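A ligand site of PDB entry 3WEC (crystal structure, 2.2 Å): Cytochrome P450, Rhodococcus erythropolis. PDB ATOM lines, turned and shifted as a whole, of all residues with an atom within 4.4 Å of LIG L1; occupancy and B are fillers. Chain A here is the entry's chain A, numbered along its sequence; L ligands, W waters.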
ATOM      1  N   LEU A  59     -34.508  -0.164   9.256  1.00  0.00           N
ATOM      2  CA  LEU A  59     -33.224   0.518   8.941  1.00  0.00           C
ATOM      3  C   LEU A  59     -33.239   1.062   7.501  1.00  0.00           C
ATOM      4  O   LEU A  59     -32.756   2.173   7.254  1.00  0.00           O
ATOM      5  CB  LEU A  59     -32.021  -0.405   9.159  1.00  0.00           C
ATOM      6  CG  LEU A  59     -31.785  -0.990  10.570  1.00  0.00           C
ATOM      7  CD1 LEU A  59     -30.774  -2.128  10.507  1.00  0.00           C
ATOM      8  CD2 LEU A  59     -31.360   0.061  11.577  1.00  0.00           C
ATOM      9  N   LYS A  66     -33.516   9.893  11.197  1.00  0.00           N
ATOM     10  CA  LYS A  66     -32.530   9.973  12.280  1.00  0.00           C
ATOM     11  C   LYS A  66     -32.354  11.389  12.818  1.00  0.00           C
ATOM     12  O   LYS A  66     -31.405  11.660  13.554  1.00  0.00           O
ATOM     13  CB  LYS A  66     -31.165   9.434  11.807  1.00  0.00           C
ATOM     14  CG  LYS A  66     -31.115   7.939  11.578  1.00  0.00           C
ATOM     15  CD  LYS A  66     -29.678   7.421  11.440  1.00  0.00           C
ATOM     16  CE  LYS A  66     -29.034   7.125  12.779  1.00  0.00           C
ATOM     17  NZ  LYS A  66     -27.838   6.259  12.634  1.00  0.00           N
ATOM     18  N   MET A 101     -24.578  13.457  10.981  1.00  0.00           N
ATOM     19  CA  MET A 101     -25.337  12.462  10.207  1.00  0.00           C
ATOM     20  C   MET A 101     -26.571  11.960  10.943  1.00  0.00           C
ATOM     21  O   MET A 101     -27.139  10.943  10.544  1.00  0.00           O
ATOM     22  CB  MET A 101     -24.451  11.249   9.854  1.00  0.00           C
ATOM     23  CG  MET A 101     -23.105  11.536   9.222  1.00  0.00           C
ATOM     24  SD  MET A 101     -23.092  11.809   7.448  1.00  0.00           S
ATOM     25  CE  MET A 101     -21.401  12.360   7.214  1.00  0.00           C
ATOM     26  N   HIS A 108     -28.763  15.020   4.748  1.00  0.00           N
ATOM     27  CA  HIS A 108     -27.877  13.884   5.015  1.00  0.00           C
ATOM     28  C   HIS A 108     -27.217  13.521   3.727  1.00  0.00           C
ATOM     29  O   HIS A 108     -26.013  13.275   3.714  1.00  0.00           O
ATOM     30  CB  HIS A 108     -28.618  12.650   5.575  1.00  0.00           C
ATOM     31  CG  HIS A 108     -27.850  11.365   5.378  1.00  0.00           C
ATOM     32  ND1 HIS A 108     -27.960  10.617   4.234  1.00  0.00           N
ATOM     33  CD2 HIS A 108     -26.921  10.740   6.161  1.00  0.00           C
ATOM     34  CE1 HIS A 108     -27.153   9.547   4.333  1.00  0.00           C
ATOM     35  NE2 HIS A 108     -26.516   9.630   5.517  1.00  0.00           N
ATOM     36  N   ARG A 112     -23.283  13.320   3.412  1.00  0.00           N
ATOM     37  CA  ARG A 112     -22.762  11.963   3.191  1.00  0.00           C
ATOM     38  C   ARG A 112     -21.882  11.897   1.983  1.00  0.00           C
ATOM     39  O   ARG A 112     -20.849  11.245   2.018  1.00  0.00           O
ATOM     40  CB  ARG A 112     -23.918  10.947   2.954  1.00  0.00           C
ATOM     41  CG  ARG A 112     -23.437   9.550   2.653  1.00  0.00           C
ATOM     42  CD  ARG A 112     -22.944   8.799   3.872  1.00  0.00           C
ATOM     43  NE  ARG A 112     -22.621   7.410   3.515  1.00  0.00           N
ATOM     44  CZ  ARG A 112     -22.731   6.354   4.313  1.00  0.00           C
ATOM     45  NH1 ARG A 112     -23.174   6.478   5.563  1.00  0.00           N
ATOM     46  NH2 ARG A 112     -22.396   5.154   3.854  1.00  0.00           N
ATOM     47  N   PHE A 119     -13.474  10.633   2.614  1.00  0.00           N
ATOM     48  CA  PHE A 119     -13.143   9.642   3.647  1.00  0.00           C
ATOM     49  C   PHE A 119     -12.429   8.447   2.988  1.00  0.00           C
ATOM     50  O   PHE A 119     -11.465   7.884   3.541  1.00  0.00           O
ATOM     51  CB  PHE A 119     -14.364   9.149   4.415  1.00  0.00           C
ATOM     52  CG  PHE A 119     -14.008   8.157   5.496  1.00  0.00           C
ATOM     53  CD1 PHE A 119     -13.559   8.620   6.738  1.00  0.00           C
ATOM     54  CD2 PHE A 119     -14.156   6.801   5.313  1.00  0.00           C
ATOM     55  CE1 PHE A 119     -13.227   7.722   7.757  1.00  0.00           C
ATOM     56  CE2 PHE A 119     -13.835   5.889   6.318  1.00  0.00           C
ATOM     57  CZ  PHE A 119     -13.359   6.341   7.552  1.00  0.00           C
ATOM     58  N   LEU A 161      -7.015   6.382  13.713  1.00  0.00           N
ATOM     59  CA  LEU A 161      -7.741   7.571  13.383  1.00  0.00           C
ATOM     60  C   LEU A 161      -6.868   8.813  13.378  1.00  0.00           C
ATOM     61  O   LEU A 161      -6.996   9.673  12.494  1.00  0.00           O
ATOM     62  CB  LEU A 161      -8.947   7.720  14.322  1.00  0.00           C
ATOM     63  CG  LEU A 161     -10.006   6.616  14.115  1.00  0.00           C
ATOM     64  CD1 LEU A 161     -11.049   6.604  15.220  1.00  0.00           C
ATOM     65  CD2 LEU A 161     -10.690   6.842  12.771  1.00  0.00           C
ATOM     66  N   LEU A 249     -17.109  13.763  14.681  1.00  0.00           N
ATOM     67  CA  LEU A 249     -18.044  12.641  14.543  1.00  0.00           C
ATOM     68  C   LEU A 249     -17.262  11.354  14.280  1.00  0.00           C
ATOM     69  O   LEU A 249     -17.484  10.293  14.893  1.00  0.00           O
ATOM     70  CB  LEU A 249     -19.077  12.906  13.439  1.00  0.00           C
ATOM     71  CG  LEU A 249     -19.705  11.657  12.807  1.00  0.00           C
ATOM     72  CD1 LEU A 249     -20.644  11.076  13.862  1.00  0.00           C
ATOM     73  CD2 LEU A 249     -20.516  12.018  11.569  1.00  0.00           C
ATOM     74  N   ILE A 250     -16.316  11.471  13.352  1.00  0.00           N
ATOM     75  CA  ILE A 250     -15.402  10.417  13.035  1.00  0.00           C
ATOM     76  C   ILE A 250     -14.513   9.968  14.200  1.00  0.00           C
ATOM     77  O   ILE A 250     -14.282   8.782  14.358  1.00  0.00           O
ATOM     78  CB  ILE A 250     -14.658  10.799  11.779  1.00  0.00           C
ATOM     79  CG1 ILE A 250     -15.687  10.497  10.622  1.00  0.00           C
ATOM     80  CG2 ILE A 250     -13.324  10.073  11.719  1.00  0.00           C
ATOM     81  CD1 ILE A 250     -15.114  10.290   9.281  1.00  0.00           C
ATOM     82  N   ALA A 253     -17.377   8.165  16.440  1.00  0.00           N
ATOM     83  CA  ALA A 253     -17.893   7.026  15.739  1.00  0.00           C
ATOM     84  C   ALA A 253     -16.989   5.820  15.746  1.00  0.00           C
ATOM     85  O   ALA A 253     -17.416   4.756  16.116  1.00  0.00           O
ATOM     86  CB  ALA A 253     -18.419   7.402  14.309  1.00  0.00           C
ATOM     87  N   GLY A 254     -15.704   5.973  15.464  1.00  0.00           N
ATOM     88  CA  GLY A 254     -14.800   4.807  15.304  1.00  0.00           C
ATOM     89  C   GLY A 254     -14.048   4.286  16.522  1.00  0.00           C
ATOM     90  O   GLY A 254     -13.300   3.289  16.431  1.00  0.00           O
ATOM     91  N   THR A 257     -16.978   1.567  19.172  1.00  0.00           N
ATOM     92  CA  THR A 257     -17.410   0.487  18.295  1.00  0.00           C
ATOM     93  C   THR A 257     -16.229  -0.467  18.029  1.00  0.00           C
ATOM     94  O   THR A 257     -16.399  -1.670  18.099  1.00  0.00           O
ATOM     95  CB  THR A 257     -17.902   1.028  16.913  1.00  0.00           C
ATOM     96  OG1 THR A 257     -16.923   1.939  16.381  1.00  0.00           O
ATOM     97  CG2 THR A 257     -19.222   1.711  17.074  1.00  0.00           C
ATOM     98  N   THR A 258     -15.044   0.085  17.742  1.00  0.00           N
ATOM     99  CA  THR A 258     -13.871  -0.722  17.396  1.00  0.00           C
ATOM    100  C   THR A 258     -13.294  -1.313  18.684  1.00  0.00           C
ATOM    101  O   THR A 258     -13.021  -2.519  18.744  1.00  0.00           O
ATOM    102  CB  THR A 258     -12.760   0.086  16.661  1.00  0.00           C
ATOM    103  OG1 THR A 258     -13.299   0.829  15.563  1.00  0.00           O
ATOM    104  CG2 THR A 258     -11.614  -0.781  16.194  1.00  0.00           C
ATOM    105  N   THR A 261     -15.418  -4.132  20.075  1.00  0.00           N
ATOM    106  CA  THR A 261     -15.291  -5.306  19.255  1.00  0.00           C
ATOM    107  C   THR A 261     -13.986  -6.087  19.437  1.00  0.00           C
ATOM    108  O   THR A 261     -13.997  -7.287  19.323  1.00  0.00           O
ATOM    109  CB  THR A 261     -15.448  -4.984  17.747  1.00  0.00           C
ATOM    110  OG1 THR A 261     -16.690  -4.300  17.566  1.00  0.00           O
ATOM    111  CG2 THR A 261     -15.456  -6.256  16.940  1.00  0.00           C
ATOM    112  N   LEU A 294     -18.633  -9.880  14.658  1.00  0.00           N
ATOM    113  CA  LEU A 294     -19.464  -8.669  14.629  1.00  0.00           C
ATOM    114  C   LEU A 294     -20.940  -9.035  14.663  1.00  0.00           C
ATOM    115  O   LEU A 294     -21.747  -8.294  15.277  1.00  0.00           O
ATOM    116  CB  LEU A 294     -19.154  -7.793  13.390  1.00  0.00           C
ATOM    117  CG  LEU A 294     -17.934  -6.883  13.381  1.00  0.00           C
ATOM    118  CD1 LEU A 294     -17.600  -6.464  11.971  1.00  0.00           C
ATOM    119  CD2 LEU A 294     -18.058  -5.621  14.207  1.00  0.00           C
ATOM    120  N   PRO A 299     -20.825  -4.483  18.557  1.00  0.00           N
ATOM    121  CA  PRO A 299     -20.480  -3.533  19.620  1.00  0.00           C
ATOM    122  C   PRO A 299     -21.676  -2.610  19.953  1.00  0.00           C
ATOM    123  O   PRO A 299     -21.805  -2.123  21.097  1.00  0.00           O
ATOM    124  CB  PRO A 299     -19.303  -2.742  19.017  1.00  0.00           C
ATOM    125  CG  PRO A 299     -19.542  -2.819  17.545  1.00  0.00           C
ATOM    126  CD  PRO A 299     -20.186  -4.147  17.272  1.00  0.00           C
ATOM    127  N   ALA A 303     -29.599   0.409  16.952  1.00  0.00           N
ATOM    128  CA  ALA A 303     -29.627   1.571  16.072  1.00  0.00           C
ATOM    129  C   ALA A 303     -30.965   2.290  16.354  1.00  0.00           C
ATOM    130  O   ALA A 303     -31.927   1.648  16.766  1.00  0.00           O
ATOM    131  CB  ALA A 303     -29.568   1.133  14.627  1.00  0.00           C
ATOM    132  N   ARG A 305     -34.284   4.956  15.183  1.00  0.00           N
ATOM    133  CA  ARG A 305     -35.034   5.639  14.133  1.00  0.00           C
ATOM    134  C   ARG A 305     -36.193   6.454  14.702  1.00  0.00           C
ATOM    135  O   ARG A 305     -36.644   6.205  15.824  1.00  0.00           O
ATOM    136  CB  ARG A 305     -35.592   4.686  13.073  1.00  0.00           C
ATOM    137  CG  ARG A 305     -34.577   4.062  12.132  1.00  0.00           C
ATOM    138  CD  ARG A 305     -33.769   5.090  11.357  1.00  0.00           C
ATOM    139  NE  ARG A 305     -32.865   4.418  10.409  1.00  0.00           N
ATOM    140  CZ  ARG A 305     -31.632   3.996  10.696  1.00  0.00           C
ATOM    141  NH1 ARG A 305     -31.094   4.139  11.917  1.00  0.00           N
ATOM    142  NH2 ARG A 305     -30.918   3.416   9.734  1.00  0.00           N
ATOM    143  N   LEU A 328     -30.252  -4.644  16.621  1.00  0.00           N
ATOM    144  CA  LEU A 328     -29.274  -5.265  15.740  1.00  0.00           C
ATOM    145  C   LEU A 328     -28.770  -6.602  16.272  1.00  0.00           C
ATOM    146  O   LEU A 328     -28.658  -7.581  15.517  1.00  0.00           O
ATOM    147  CB  LEU A 328     -28.086  -4.310  15.560  1.00  0.00           C
ATOM    148  CG  LEU A 328     -28.317  -2.839  15.206  1.00  0.00           C
ATOM    149  CD1 LEU A 328     -26.954  -2.180  15.114  1.00  0.00           C
ATOM    150  CD2 LEU A 328     -29.028  -2.660  13.872  1.00  0.00           C
ATOM    151  N   SER A 353     -24.961  -5.511  11.948  1.00  0.00           N
ATOM    152  CA  SER A 353     -24.107  -4.740  12.859  1.00  0.00           C
ATOM    153  C   SER A 353     -23.652  -3.335  12.380  1.00  0.00           C
ATOM    154  O   SER A 353     -23.269  -2.501  13.198  1.00  0.00           O
ATOM    155  CB  SER A 353     -22.943  -5.593  13.382  1.00  0.00           C
ATOM    156  OG  SER A 353     -23.500  -6.731  13.984  1.00  0.00           O
ATOM    157  N   TYR A 354     -23.735  -3.105  11.065  1.00  0.00           N
ATOM    158  CA  TYR A 354     -23.386  -1.828  10.478  1.00  0.00           C
ATOM    159  C   TYR A 354     -24.598  -0.998  10.009  1.00  0.00           C
ATOM    160  O   TYR A 354     -24.428   0.078   9.430  1.00  0.00           O
ATOM    161  CB  TYR A 354     -22.436  -2.064   9.320  1.00  0.00           C
ATOM    162  CG  TYR A 354     -21.001  -2.473   9.631  1.00  0.00           C
ATOM    163  CD1 TYR A 354     -20.178  -1.671  10.472  1.00  0.00           C
ATOM    164  CD2 TYR A 354     -20.423  -3.647   9.055  1.00  0.00           C
ATOM    165  CE1 TYR A 354     -18.847  -1.997  10.731  1.00  0.00           C
ATOM    166  CE2 TYR A 354     -19.076  -3.977   9.300  1.00  0.00           C
ATOM    167  CZ  TYR A 354     -18.309  -3.144  10.171  1.00  0.00           C
ATOM    168  OH  TYR A 354     -17.002  -3.413  10.430  1.00  0.00           O
ATOM    169  N   GLY A 355     -25.823  -1.473  10.285  1.00  0.00           N
ATOM    170  CA  GLY A 355     -27.020  -0.770   9.889  1.00  0.00           C
ATOM    171  C   GLY A 355     -27.254  -1.182   8.437  1.00  0.00           C
ATOM    172  O   GLY A 355     -26.494  -2.004   7.922  1.00  0.00           O
ATOM    173  N   ARG A 356     -28.279  -0.647   7.790  1.00  0.00           N
ATOM    174  CA  ARG A 356     -28.580  -0.946   6.374  1.00  0.00           C
ATOM    175  C   ARG A 356     -29.226   0.280   5.735  1.00  0.00           C
ATOM    176  O   ARG A 356     -29.918   1.063   6.418  1.00  0.00           O
ATOM    177  CB  ARG A 356     -29.532  -2.155   6.254  1.00  0.00           C
ATOM    178  CG  ARG A 356     -28.917  -3.454   5.706  1.00  0.00           C
ATOM    179  CD  ARG A 356     -28.562  -4.360   6.857  1.00  0.00           C
ATOM    180  NE  ARG A 356     -27.996  -5.669   6.538  1.00  0.00           N
ATOM    181  CZ  ARG A 356     -28.727  -6.782   6.433  1.00  0.00           C
ATOM    182  NH1 ARG A 356     -30.052  -6.703   6.530  1.00  0.00           N
ATOM    183  NH2 ARG A 356     -28.141  -7.961   6.194  1.00  0.00           N
ATOM    184  N   ILE A 358     -29.189   4.004   3.758  1.00  0.00           N
ATOM    185  CA  ILE A 358     -28.460   5.232   3.432  1.00  0.00           C
ATOM    186  C   ILE A 358     -27.496   5.561   4.556  1.00  0.00           C
ATOM    187  O   ILE A 358     -26.487   6.172   4.274  1.00  0.00           O
ATOM    188  CB  ILE A 358     -29.359   6.474   3.127  1.00  0.00           C
ATOM    189  CG1 ILE A 358     -30.424   6.668   4.216  1.00  0.00           C
ATOM    190  CG2 ILE A 358     -29.985   6.360   1.718  1.00  0.00           C
ATOM    191  CD1 ILE A 358     -31.234   7.938   4.139  1.00  0.00           C
ATOM    192  N   HIS A 359     -27.782   5.098   5.774  1.00  0.00           N
ATOM    193  CA  HIS A 359     -26.918   5.355   6.923  1.00  0.00           C
ATOM    194  C   HIS A 359     -25.964   4.221   7.190  1.00  0.00           C
ATOM    195  O   HIS A 359     -25.287   4.227   8.195  1.00  0.00           O
ATOM    196  CB  HIS A 359     -27.723   5.677   8.190  1.00  0.00           C
ATOM    197  CG  HIS A 359     -28.625   6.907   8.083  1.00  0.00           C
ATOM    198  ND1 HIS A 359     -28.198   8.162   8.284  1.00  0.00           N
ATOM    199  CD2 HIS A 359     -29.978   7.015   7.737  1.00  0.00           C
ATOM    200  CE1 HIS A 359     -29.214   9.012   8.192  1.00  0.00           C
ATOM    201  NE2 HIS A 359     -30.312   8.314   7.834  1.00  0.00           N
ATOM    202  N   CYS A 361     -23.049   2.073   8.029  1.00  0.00           N
ATOM    203  CA  CYS A 361     -21.817   2.615   8.634  1.00  0.00           C
ATOM    204  C   CYS A 361     -20.723   3.122   7.679  1.00  0.00           C
ATOM    205  O   CYS A 361     -19.898   2.381   7.316  1.00  0.00           O
ATOM    206  CB  CYS A 361     -21.109   1.575   9.461  1.00  0.00           C
ATOM    207  SG  CYS A 361     -19.585   2.317  10.219  1.00  0.00           S
ATOM    208  N   LEU A 362     -20.622   4.396   7.355  1.00  0.00           N
ATOM    209  CA  LEU A 362     -19.495   4.873   6.554  1.00  0.00           C
ATOM    210  C   LEU A 362     -18.072   4.298   6.825  1.00  0.00           C
ATOM    211  O   LEU A 362     -17.302   4.110   5.862  1.00  0.00           O
ATOM    212  CB  LEU A 362     -19.489   6.413   6.533  1.00  0.00           C
ATOM    213  CG  LEU A 362     -18.495   7.092   5.574  1.00  0.00           C
ATOM    214  CD1 LEU A 362     -18.988   6.873   4.153  1.00  0.00           C
ATOM    215  CD2 LEU A 362     -18.361   8.570   5.842  1.00  0.00           C
ATOM    216  N   GLY A 363     -17.696   4.074   8.105  1.00  0.00           N
ATOM    217  CA  GLY A 363     -16.380   3.524   8.433  1.00  0.00           C
ATOM    218  C   GLY A 363     -16.233   2.010   8.331  1.00  0.00           C
ATOM    219  O   GLY A 363     -15.262   1.460   8.812  1.00  0.00           O
ATOM    220  N   LEU A 366     -13.070   0.303   6.942  1.00  0.00           N
ATOM    221  CA  LEU A 366     -11.925   0.627   7.779  1.00  0.00           C
ATOM    222  C   LEU A 366     -11.967  -0.170   9.063  1.00  0.00           C
ATOM    223  O   LEU A 366     -10.984  -0.758   9.445  1.00  0.00           O
ATOM    224  CB  LEU A 366     -11.904   2.146   8.142  1.00  0.00           C
ATOM    225  CG  LEU A 366     -10.812   2.639   9.137  1.00  0.00           C
ATOM    226  CD1 LEU A 366      -9.392   2.356   8.620  1.00  0.00           C
ATOM    227  CD2 LEU A 366     -10.991   4.140   9.262  1.00  0.00           C
ATOM    228  N   ALA A 367     -13.098  -0.156   9.755  1.00  0.00           N
ATOM    229  CA  ALA A 367     -13.298  -1.048  10.896  1.00  0.00           C
ATOM    230  C   ALA A 367     -12.962  -2.507  10.525  1.00  0.00           C
ATOM    231  O   ALA A 367     -12.309  -3.188  11.283  1.00  0.00           O
ATOM    232  CB  ALA A 367     -14.718  -0.912  11.462  1.00  0.00           C
ATOM    233  N   MET A 370      -9.173  -2.870  10.087  1.00  0.00           N
ATOM    234  CA  MET A 370      -8.579  -2.873  11.432  1.00  0.00           C
ATOM    235  C   MET A 370      -8.744  -4.239  12.119  1.00  0.00           C
ATOM    236  O   MET A 370      -7.797  -4.776  12.694  1.00  0.00           O
ATOM    237  CB  MET A 370      -9.206  -1.810  12.374  1.00  0.00           C
ATOM    238  CG  MET A 370      -8.669  -0.394  12.162  1.00  0.00           C
ATOM    239  SD  MET A 370      -9.267   0.810  13.356  1.00  0.00           S
ATOM    240  CE  MET A 370     -10.992   0.938  12.855  1.00  0.00           C
HETATM  241  C1  LIG L   1     -22.971   4.794  11.474  1.00  0.00           C
HETATM  242  C2  LIG L   1     -21.760   0.435  13.509  1.00  0.00           C
HETATM  243  C3  LIG L   1     -16.996   1.487  12.945  1.00  0.00           C
HETATM  244  C4  LIG L   1     -18.270   5.996  11.064  1.00  0.00           C
HETATM  245  C5  LIG L   1     -22.970   3.506  12.127  1.00  0.00           C
HETATM  246  C6  LIG L   1     -24.229   2.891  12.630  1.00  0.00           C
HETATM  247  C7  LIG L   1     -23.851   1.626  13.205  1.00  0.00           C
HETATM  248  C8  LIG L   1     -22.400   1.605  13.043  1.00  0.00           C
HETATM  249  C9  LIG L   1     -24.772   0.564  13.871  1.00  0.00           C
HETATM  250  C10 LIG L   1     -25.697   3.333  12.579  1.00  0.00           C
HETATM  251  C11 LIG L   1     -26.185   2.804  11.217  1.00  0.00           C
HETATM  252  C12 LIG L   1     -27.711   2.925  11.063  1.00  0.00           C
HETATM  253  O1  LIG L   1     -28.380   3.782  11.723  1.00  0.00           O
HETATM  254  O2  LIG L   1     -28.280   2.171  10.227  1.00  0.00           O
HETATM  255  C13 LIG L   1     -20.302   0.377  13.535  1.00  0.00           C
HETATM  256  C14 LIG L   1     -19.668  -0.878  13.944  1.00  0.00           C
HETATM  257  C15 LIG L   1     -18.281  -0.511  13.798  1.00  0.00           C
HETATM  258  C16 LIG L   1     -18.264   0.862  13.318  1.00  0.00           C
HETATM  259  C17 LIG L   1     -20.235  -2.171  14.456  1.00  0.00           C
HETATM  260  C18 LIG L   1     -17.168  -1.449  14.111  1.00  0.00           C
HETATM  261  C19 LIG L   1     -16.140  -1.020  14.789  1.00  0.00           C
HETATM  262  C20 LIG L   1     -16.929   2.798  12.342  1.00  0.00           C
HETATM  263  C21 LIG L   1     -15.658   3.510  12.165  1.00  0.00           C
HETATM  264  C22 LIG L   1     -16.072   4.829  11.623  1.00  0.00           C
HETATM  265  C23 LIG L   1     -17.513   4.840  11.527  1.00  0.00           C
HETATM  266  C24 LIG L   1     -14.298   2.963  12.488  1.00  0.00           C
HETATM  267  C25 LIG L   1     -15.217   6.007  11.261  1.00  0.00           C
HETATM  268  C26 LIG L   1     -13.914   5.941  11.151  1.00  0.00           C
HETATM  269  C27 LIG L   1     -19.735   6.094  11.073  1.00  0.00           C
HETATM  270  C28 LIG L   1     -20.391   7.252  10.457  1.00  0.00           C
HETATM  271  C29 LIG L   1     -21.816   6.920  10.578  1.00  0.00           C
HETATM  272  C30 LIG L   1     -21.787   5.575  11.176  1.00  0.00           C
HETATM  273  C31 LIG L   1     -19.739   8.499   9.916  1.00  0.00           C
HETATM  274  C32 LIG L   1     -23.002   7.745  10.166  1.00  0.00           C
HETATM  275  C33 LIG L   1     -23.440   7.222   8.776  1.00  0.00           C
HETATM  276  C34 LIG L   1     -24.606   7.963   8.207  1.00  0.00           C
HETATM  277  O3  LIG L   1     -24.616   8.132   6.956  1.00  0.00           O
HETATM  278  O4  LIG L   1     -25.510   8.391   8.993  1.00  0.00           O
HETATM  279  N1  LIG L   1     -21.778   2.677  12.260  1.00  0.00           N
HETATM  280  N2  LIG L   1     -19.491   1.390  13.096  1.00  0.00           N
HETATM  281  N3  LIG L   1     -18.045   3.562  11.910  1.00  0.00           N
HETATM  282  N4  LIG L   1     -20.555   5.078  11.450  1.00  0.00           N
HETATM  283 FE1  LIG L   1     -19.901   3.290  12.344  1.00  0.00          FE
HETATM  284  O1  LG2 L   2     -26.560   6.074  15.188  1.00  0.00           O
HETATM  285  C1  LG2 L   2     -25.374   5.670  15.213  1.00  0.00           C
HETATM  286  C2  LG2 L   2     -24.319   6.562  14.705  1.00  0.00           C
HETATM  287  C3  LG2 L   2     -24.619   7.833  14.235  1.00  0.00           C
HETATM  288  C4  LG2 L   2     -23.607   8.668  13.770  1.00  0.00           C
HETATM  289  C5  LG2 L   2     -22.284   8.190  13.833  1.00  0.00           C
HETATM  290  C6  LG2 L   2     -21.933   6.925  14.317  1.00  0.00           C
HETATM  291  C7  LG2 L   2     -22.911   6.064  14.780  1.00  0.00           C
HETATM  292  N1  LG2 L   2     -22.595   4.831  15.291  1.00  0.00           N
HETATM  293  C8  LG2 L   2     -23.514   3.955  15.750  1.00  0.00           C
HETATM  294  C9  LG2 L   2     -23.101   2.599  16.302  1.00  0.00           C
HETATM  295  C10 LG2 L   2     -24.962   4.332  15.739  1.00  0.00           C
HETATM  296  C11 LG2 L   2     -25.998   3.376  16.287  1.00  0.00           C
HETATM  297  C12 LG2 L   2     -25.791   3.235  17.791  1.00  0.00           C
HETATM  298  C13 LG2 L   2     -25.705   4.106  18.840  1.00  0.00           C
HETATM  299  C14 LG2 L   2     -25.760   5.622  18.758  1.00  0.00           C
HETATM  300  C15 LG2 L   2     -25.482   3.433  20.172  1.00  0.00           C
HETATM  301  C16 LG2 L   2     -26.567   3.619  21.241  1.00  0.00           C
HETATM  302  C17 LG2 L   2     -27.502   4.761  20.952  1.00  0.00           C
HETATM  303  C18 LG2 L   2     -28.687   4.980  21.559  1.00  0.00           C
HETATM  304  C19 LG2 L   2     -29.262   4.145  22.675  1.00  0.00           C
HETATM  305  C20 LG2 L   2     -29.464   6.207  21.122  1.00  0.00           C
HETATM  306  C21 LG2 L   2     -30.360   6.005  19.900  1.00  0.00           C
HETATM  307  O2  LG2 L   2     -30.787   7.315  19.517  1.00  0.00           O
HETATM  308  C22 LG2 L   2     -29.715   5.436  18.655  1.00  0.00           C
HETATM  309  C23 LG2 L   2     -29.294   6.104  17.544  1.00  0.00           C
HETATM  310  C24 LG2 L   2     -28.720   5.271  16.451  1.00  0.00           C
HETATM  311  C25 LG2 L   2     -29.334   7.601  17.273  1.00  0.00           C
HETATM  312  O   HOH W   1     -23.133  -3.110  16.127  1.00  0.00           O
HETATM  313  O   HOH W   2     -19.864   3.846  14.757  1.00  0.00           O
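FE1 of LIG L1 is bound by SG of Cys 361.
The guanidinium group (NH1) of Arg 112 is in salt-bridge range of an oxygen (O3) of LIG L1.
An oxygen (O1) of LIG L1 lies within salt-bridge range of the side-chain amino group (NZ) of Lys 66 (2.7 Å).
NH1 of Arg 305 lies within salt-bridge range of O1 of LIG L1 (2.7 Å).
A ring nitrogen (ND1) of His 359 is in hydrogen-bond range of an oxygen (O4) of LIG L1, 2.8 Å away.
O3 of LIG L1 sits at hydrogen-bond distance from NE2 of His 108 (2.8 Å).
An oxygen (O1) of LG2 L2 lies within hydrogen-bond range of the side-chain amino group (NZ) of Lys 66 (2.9 Å).
The backbone NH (N) of Cys 361 is in hydrogen-bond range of the backbone carbonyl oxygen (O) of Tyr 354 (2.8 Å).
The side-chain sulfur of Cys 361 lies close to the backbone NH of Gly 363 (3.3 Å).
NH2 of Arg 305 sits at hydrogen-bond distance from O of Leu 59 (3.3 Å).
The backbone carbonyl oxygen (O) of Ala 253 is in hydrogen-bond range of the side-chain hydroxyl (OG1) of Thr 257 (2.9 Å).
The backbone carbonyl oxygen of Thr 257 is in hydrogen-bond range of the side-chain hydroxyl of Thr 261 (2.7 Å).
O of Leu 294 is in hydrogen-bond range of OG of Ser 353.
O of Gly 254 lies within hydrogen-bond range of OG1 of Thr 258, 2.6 Å away.
An oxygen (O4) of LIG L1 sits close to the backbone carbonyl oxygen of Met 101, at 3.4 Å.
Residues that only touch LIG L1: Gly 355 (3.2 Å), Pro 299 (3.2 Å), Thr 257 (3.3 Å), Ser 353 (3.3 Å), Thr 258 (3.3 Å), Gly 254 (3.4 Å), Tyr 354 (3.5 Å), Gly 363 (3.5 Å), Ala 253 (3.5 Å), Ala 367 (3.6 Å), Phe 119 (3.7 Å), Leu 161 (3.7 Å), Leu 328 (3.7 Å), Arg 356 (3.7 Å), Ile 358 (3.8 Å), Met 370 (3.9 Å), Leu 366 (3.9 Å), Leu 249 (3.96 Å), Leu 59 (3.97 Å) and Leu 362 (3.98 Å).
Hydrophobic or aromatic side chains within 4 Å of LIG L1: Leu 59, Met 101, His 108, Phe 119, Leu 161, Leu 249, Ala 253, Pro 299, Leu 328, Tyr 354, His 359, Leu 362, Leu 366, Ala 367 and Met 370.
Within 4 Å of LIG L1: Leu 59, Lys 66, Met 101, His 108, Arg 112, Phe 119, Leu 161, Leu 249, Ala 253, Gly 254, Thr 257, Thr 258, Pro 299, Arg 305, Leu 328, Ser 353, Tyr 354, Gly 355, Arg 356, Ile 358, His 359, Cys 361, Leu 362, Gly 363, Leu 366, Ala 367 and Met 370.
Water W2 bridges the backbone carbonyl oxygen of Ala 253 and a nitrogen (N1) of LG2 L2.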
